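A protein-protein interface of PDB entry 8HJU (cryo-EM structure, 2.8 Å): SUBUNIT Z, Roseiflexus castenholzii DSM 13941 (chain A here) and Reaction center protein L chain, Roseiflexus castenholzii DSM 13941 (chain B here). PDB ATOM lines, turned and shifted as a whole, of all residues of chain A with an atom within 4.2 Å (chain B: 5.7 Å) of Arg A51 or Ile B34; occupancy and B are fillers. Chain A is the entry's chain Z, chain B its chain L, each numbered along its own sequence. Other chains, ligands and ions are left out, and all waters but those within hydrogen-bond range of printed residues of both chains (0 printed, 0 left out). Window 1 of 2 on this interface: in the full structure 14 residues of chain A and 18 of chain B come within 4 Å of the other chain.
The guanidinium group (NE) of Arg A51 lies within hydrogen-bond range of the backbone carbonyl oxygen (O) of Ile B34 (3.0 Å). The backbone carbonyl oxygen (O) of Glu B32 sits at hydrogen-bond distance from the backbone NH (N) of Arg A51, 2.9 Å away. The side-chain carboxylate of Glu B32 lies close to the side-chain carboxylate of Asp A53 (3.3 Å). The backbone NH of Ile B34 sits at hydrogen-bond distance from the backbone carbonyl oxygen of Tyr A49.
O of Ser A47 is in hydrogen-bond range of NH2 of Arg A51 (2.6 Å). The backbone carbonyl oxygen (O) of Ala A45 sits at hydrogen-bond distance from the guanidinium group (NH2) of Arg A51, at 3.3 Å. The guanidinium group (NH1) of Arg A51 lies within hydrogen-bond range of the side-chain hydroxyl (OH) of Tyr A49 (3.4 Å). The backbone carbonyl oxygen of Ala A45 lies within hydrogen-bond range of the side-chain hydroxyl of Tyr A49, 3.3 Å away.
Among the printed residues, pairs that only touch across the chains: Ala A45 with Phe B36 (3.9 Å), Ala A48 with Val B33 (3.7 Å), Ala A48 with Ile B34 (3.8 Å), Tyr A49 with Glu B32 (3.6 Å), Tyr A49 with Val B33 (3.5 Å), Leu A50 with Ala B31 (3.5 Å), Leu A50 with Glu B32 (3.4 Å), Leu A50 with Val B33 (3.96 Å), Arg A51 with Ala B31 (3.5 Å), Arg A51 with Phe B36 (3.9 Å), Arg A51 with Ile B39 (3.6 Å), Leu A52 with Ser B30 (3.4 Å), Leu A52 with Ala B31 (3.9 Å), Leu A52 with Ile B34 (3.7 Å) and Asp A53 with Ile B34 (3.3 Å).
Ser A47 touches none of the printed residues of chain B. Of the printed residues of chain B, Ala A48 touches Val B33 (3.7 Å) and Ile B34 (3.8 Å). Of the printed residues of chain B, Tyr A49 touches Glu B32 (3.6 Å), Val B33 (3.5 Å) and Ile B34 (3.3 Å). Of the printed residues of chain B, Leu A50 touches Ala B31, Glu B32 and Val B33. Arg A51 touches five residues of chain B. Of the printed residues of chain B, Leu A52 touches Ser B30, Ala B31 and Ile B34. Printed residues of chain A within 4 Å of Ala B31: Leu A50, Arg A51 and Leu A52. Ile B34 touches five residues of chain A. The nearest residue of chain B that does not touch Arg A51 is Pro B35 (4.4 Å). The nearest printed residue of chain B that does not touch Leu A50 is Ile B34 (5.0 Å).
Hydrophobic or aromatic side chains of chain A that line the printed part of chain B: Ala A48, Leu A50 and Leu A52. Printed residues of chain B that touch a printed residue of chain A: Ser B30, Ala B31, Glu B32, Val B33, Ile B34, Phe B36 and Ile B39. Hydrophobic or aromatic side chains of chain B within 4 Å of the printed part of chain A: Ala B31, Val B33, Ile B34, Phe B36 and Ile B39. Among the printed residues, 19 pairs touch across the chains. Among the printed residues, no Asp or Glu carboxylate lies within 4 Å of a Lys or Arg side-chain nitrogen of the other chain.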
ATOM      1  N   ALA A  45      -7.352  -2.346 -15.056  1.00  0.00           N
ATOM      2  CA  ALA A  45      -8.134  -2.536 -16.270  1.00  0.00           C
ATOM      3  C   ALA A  45      -9.076  -1.371 -16.545  1.00  0.00           C
ATOM      4  O   ALA A  45      -9.369  -1.082 -17.706  1.00  0.00           O
ATOM      5  CB  ALA A  45      -8.921  -3.837 -16.184  1.00  0.00           C
ATOM      6  N   SER A  47      -8.449   1.771 -15.384  1.00  0.00           N
ATOM      7  CA  SER A  47      -7.728   3.025 -15.506  1.00  0.00           C
ATOM      8  C   SER A  47      -7.724   3.493 -16.960  1.00  0.00           C
ATOM      9  O   SER A  47      -8.133   2.780 -17.877  1.00  0.00           O
ATOM     10  CB  SER A  47      -6.303   2.878 -14.984  1.00  0.00           C
ATOM     11  OG  SER A  47      -5.571   1.961 -15.767  1.00  0.00           O
ATOM     12  N   ALA A  48      -7.256   4.717 -17.167  1.00  0.00           N
ATOM     13  CA  ALA A  48      -7.198   5.317 -18.490  1.00  0.00           C
ATOM     14  C   ALA A  48      -5.817   5.093 -19.088  1.00  0.00           C
ATOM     15  O   ALA A  48      -4.808   5.495 -18.502  1.00  0.00           O
ATOM     16  CB  ALA A  48      -7.520   6.807 -18.427  1.00  0.00           C
ATOM     17  N   TYR A  49      -5.777   4.448 -20.247  1.00  0.00           N
ATOM     18  CA  TYR A  49      -4.537   4.212 -20.961  1.00  0.00           C
ATOM     19  C   TYR A  49      -4.854   4.188 -22.447  1.00  0.00           C
ATOM     20  O   TYR A  49      -6.000   4.365 -22.857  1.00  0.00           O
ATOM     21  CB  TYR A  49      -3.863   2.924 -20.493  1.00  0.00           C
ATOM     22  CG  TYR A  49      -4.772   1.728 -20.392  1.00  0.00           C
ATOM     23  CD1 TYR A  49      -5.255   1.109 -21.525  1.00  0.00           C
ATOM     24  CD2 TYR A  49      -5.118   1.202 -19.166  1.00  0.00           C
ATOM     25  CE1 TYR A  49      -6.064   0.022 -21.441  1.00  0.00           C
ATOM     26  CE2 TYR A  49      -5.930   0.112 -19.073  1.00  0.00           C
ATOM     27  CZ  TYR A  49      -6.401  -0.475 -20.214  1.00  0.00           C
ATOM     28  OH  TYR A  49      -7.218  -1.571 -20.138  1.00  0.00           O
ATOM     29  N   LEU A  50      -3.831   3.962 -23.259  1.00  0.00           N
ATOM     30  CA  LEU A  50      -4.005   4.048 -24.701  1.00  0.00           C
ATOM     31  C   LEU A  50      -4.962   2.966 -25.175  1.00  0.00           C
ATOM     32  O   LEU A  50      -4.629   1.780 -25.169  1.00  0.00           O
ATOM     33  CB  LEU A  50      -2.663   3.931 -25.411  1.00  0.00           C
ATOM     34  CG  LEU A  50      -1.761   5.151 -25.288  1.00  0.00           C
ATOM     35  CD1 LEU A  50      -0.316   4.753 -25.456  1.00  0.00           C
ATOM     36  CD2 LEU A  50      -2.144   6.206 -26.297  1.00  0.00           C
ATOM     37  N   ARG A  51      -6.149   3.377 -25.591  1.00  0.00           N
ATOM     38  CA  ARG A  51      -7.082   2.514 -26.286  1.00  0.00           C
ATOM     39  C   ARG A  51      -7.350   3.100 -27.661  1.00  0.00           C
ATOM     40  O   ARG A  51      -7.123   4.284 -27.902  1.00  0.00           O
ATOM     41  CB  ARG A  51      -8.401   2.370 -25.518  1.00  0.00           C
ATOM     42  CG  ARG A  51      -8.234   2.161 -24.034  1.00  0.00           C
ATOM     43  CD  ARG A  51      -9.446   2.637 -23.266  1.00  0.00           C
ATOM     44  NE  ARG A  51      -9.258   2.518 -21.825  1.00  0.00           N
ATOM     45  CZ  ARG A  51      -9.308   1.371 -21.169  1.00  0.00           C
ATOM     46  NH1 ARG A  51      -9.538   0.248 -21.826  1.00  0.00           N
ATOM     47  NH2 ARG A  51      -9.126   1.347 -19.863  1.00  0.00           N
ATOM     48  N   LEU A  52      -7.822   2.260 -28.567  1.00  0.00           N
ATOM     49  CA  LEU A  52      -8.349   2.753 -29.827  1.00  0.00           C
ATOM     50  C   LEU A  52      -9.734   3.316 -29.575  1.00  0.00           C
ATOM     51  O   LEU A  52     -10.580   2.644 -28.978  1.00  0.00           O
ATOM     52  CB  LEU A  52      -8.414   1.637 -30.862  1.00  0.00           C
ATOM     53  CG  LEU A  52      -7.085   0.996 -31.244  1.00  0.00           C
ATOM     54  CD1 LEU A  52      -7.282   0.072 -32.420  1.00  0.00           C
ATOM     55  CD2 LEU A  52      -6.060   2.065 -31.558  1.00  0.00           C
ATOM     56  N   ASP A  53      -9.971   4.546 -30.012  1.00  0.00           N
ATOM     57  CA  ASP A  53     -11.267   5.155 -29.763  1.00  0.00           C
ATOM     58  C   ASP A  53     -12.363   4.300 -30.393  1.00  0.00           C
ATOM     59  O   ASP A  53     -12.271   3.957 -31.574  1.00  0.00           O
ATOM     60  CB  ASP A  53     -11.343   6.579 -30.303  1.00  0.00           C
ATOM     61  CG  ASP A  53     -12.628   7.261 -29.914  1.00  0.00           C
ATOM     62  OD1 ASP A  53     -12.954   7.262 -28.708  1.00  0.00           O
ATOM     63  OD2 ASP A  53     -13.338   7.754 -30.806  1.00  0.00           O
ATOM     64  N   SER B  30      -2.939   5.071 -33.718  1.00  0.00           N
ATOM     65  CA  SER B  30      -4.181   5.811 -33.534  1.00  0.00           C
ATOM     66  C   SER B  30      -4.613   5.895 -32.079  1.00  0.00           C
ATOM     67  O   SER B  30      -5.638   6.517 -31.789  1.00  0.00           O
ATOM     68  CB  SER B  30      -5.301   5.164 -34.356  1.00  0.00           C
ATOM     69  OG  SER B  30      -5.153   3.752 -34.392  1.00  0.00           O
ATOM     70  N   ALA B  31      -3.861   5.295 -31.166  1.00  0.00           N
ATOM     71  CA  ALA B  31      -4.300   5.194 -29.785  1.00  0.00           C
ATOM     72  C   ALA B  31      -4.301   6.552 -29.103  1.00  0.00           C
ATOM     73  O   ALA B  31      -3.398   7.367 -29.297  1.00  0.00           O
ATOM     74  CB  ALA B  31      -3.398   4.233 -29.018  1.00  0.00           C
ATOM     75  N   GLU B  32      -5.332   6.787 -28.298  1.00  0.00           N
ATOM     76  CA  GLU B  32      -5.377   7.919 -27.392  1.00  0.00           C
ATOM     77  C   GLU B  32      -5.699   7.391 -26.008  1.00  0.00           C
ATOM     78  O   GLU B  32      -6.251   6.302 -25.857  1.00  0.00           O
ATOM     79  CB  GLU B  32      -6.411   8.960 -27.831  1.00  0.00           C
ATOM     80  CG  GLU B  32      -7.692   8.363 -28.380  1.00  0.00           C
ATOM     81  CD  GLU B  32      -8.883   9.276 -28.212  1.00  0.00           C
ATOM     82  OE1 GLU B  32      -8.693  10.494 -28.029  1.00  0.00           O
ATOM     83  OE2 GLU B  32     -10.019   8.768 -28.256  1.00  0.00           O
ATOM     84  N   VAL B  33      -5.329   8.155 -24.988  1.00  0.00           N
ATOM     85  CA  VAL B  33      -5.650   7.783 -23.616  1.00  0.00           C
ATOM     86  C   VAL B  33      -7.137   8.040 -23.407  1.00  0.00           C
ATOM     87  O   VAL B  33      -7.570   9.189 -23.317  1.00  0.00           O
ATOM     88  CB  VAL B  33      -4.804   8.555 -22.604  1.00  0.00           C
ATOM     89  CG1 VAL B  33      -5.147   8.113 -21.198  1.00  0.00           C
ATOM     90  CG2 VAL B  33      -3.341   8.334 -22.887  1.00  0.00           C
ATOM     91  N   ILE B  34      -7.916   6.963 -23.406  1.00  0.00           N
ATOM     92  CA  ILE B  34      -9.343   7.081 -23.226  1.00  0.00           C
ATOM     93  C   ILE B  34      -9.796   6.533 -21.912  1.00  0.00           C
ATOM     94  O   ILE B  34      -9.419   5.466 -21.527  1.00  0.00           O
ATOM     95  CB  ILE B  34     -10.097   6.328 -24.326  1.00  0.00           C
ATOM     96  CG1 ILE B  34      -9.499   6.632 -25.673  1.00  0.00           C
ATOM     97  CG2 ILE B  34     -11.570   6.678 -24.346  1.00  0.00           C
ATOM     98  CD1 ILE B  34     -10.011   5.691 -26.713  1.00  0.00           C
ATOM     99  N   PRO B  35     -10.654   7.259 -21.224  1.00  0.00           N
ATOM    100  CA  PRO B  35     -11.228   6.701 -20.011  1.00  0.00           C
ATOM    101  C   PRO B  35     -12.122   5.457 -20.273  1.00  0.00           C
ATOM    102  O   PRO B  35     -12.745   5.374 -21.313  1.00  0.00           O
ATOM    103  CB  PRO B  35     -12.049   7.856 -19.502  1.00  0.00           C
ATOM    104  CG  PRO B  35     -11.357   9.069 -19.970  1.00  0.00           C
ATOM    105  CD  PRO B  35     -10.867   8.709 -21.328  1.00  0.00           C
ATOM    106  N   PHE B  36     -12.173   4.494 -19.351  1.00  0.00           N
ATOM    107  CA  PHE B  36     -13.065   3.339 -19.453  1.00  0.00           C
ATOM    108  C   PHE B  36     -14.520   3.743 -19.509  1.00  0.00           C
ATOM    109  O   PHE B  36     -15.266   3.185 -20.274  1.00  0.00           O
ATOM    110  CB  PHE B  36     -12.814   2.357 -18.307  1.00  0.00           C
ATOM    111  CG  PHE B  36     -13.416   1.008 -18.517  1.00  0.00           C
ATOM    112  CD1 PHE B  36     -12.779   0.071 -19.301  1.00  0.00           C
ATOM    113  CD2 PHE B  36     -14.621   0.677 -17.937  1.00  0.00           C
ATOM    114  CE1 PHE B  36     -13.332  -1.172 -19.501  1.00  0.00           C
ATOM    115  CE2 PHE B  36     -15.181  -0.560 -18.137  1.00  0.00           C
ATOM    116  CZ  PHE B  36     -14.533  -1.492 -18.914  1.00  0.00           C
ATOM    117  N   ILE B  38     -15.817   6.043 -20.961  1.00  0.00           N
ATOM    118  CA  ILE B  38     -16.142   6.318 -22.358  1.00  0.00           C
ATOM    119  C   ILE B  38     -16.349   5.018 -23.123  1.00  0.00           C
ATOM    120  O   ILE B  38     -17.332   4.862 -23.861  1.00  0.00           O
ATOM    121  CB  ILE B  38     -15.042   7.179 -23.000  1.00  0.00           C
ATOM    122  CG1 ILE B  38     -14.923   8.524 -22.280  1.00  0.00           C
ATOM    123  CG2 ILE B  38     -15.317   7.374 -24.474  1.00  0.00           C
ATOM    124  CD1 ILE B  38     -16.245   9.177 -21.975  1.00  0.00           C
ATOM    125  N   ILE B  39     -15.427   4.068 -22.960  1.00  0.00           N
ATOM    126  CA  ILE B  39     -15.568   2.757 -23.584  1.00  0.00           C
ATOM    127  C   ILE B  39     -16.868   2.095 -23.150  1.00  0.00           C
ATOM    128  O   ILE B  39     -17.588   1.511 -23.967  1.00  0.00           O
ATOM    129  CB  ILE B  39     -14.354   1.875 -23.245  1.00  0.00           C
ATOM    130  CG1 ILE B  39     -13.051   2.572 -23.640  1.00  0.00           C
ATOM    131  CG2 ILE B  39     -14.473   0.527 -23.911  1.00  0.00           C
ATOM    132  CD1 ILE B  39     -12.991   2.999 -25.079  1.00  0.00           C
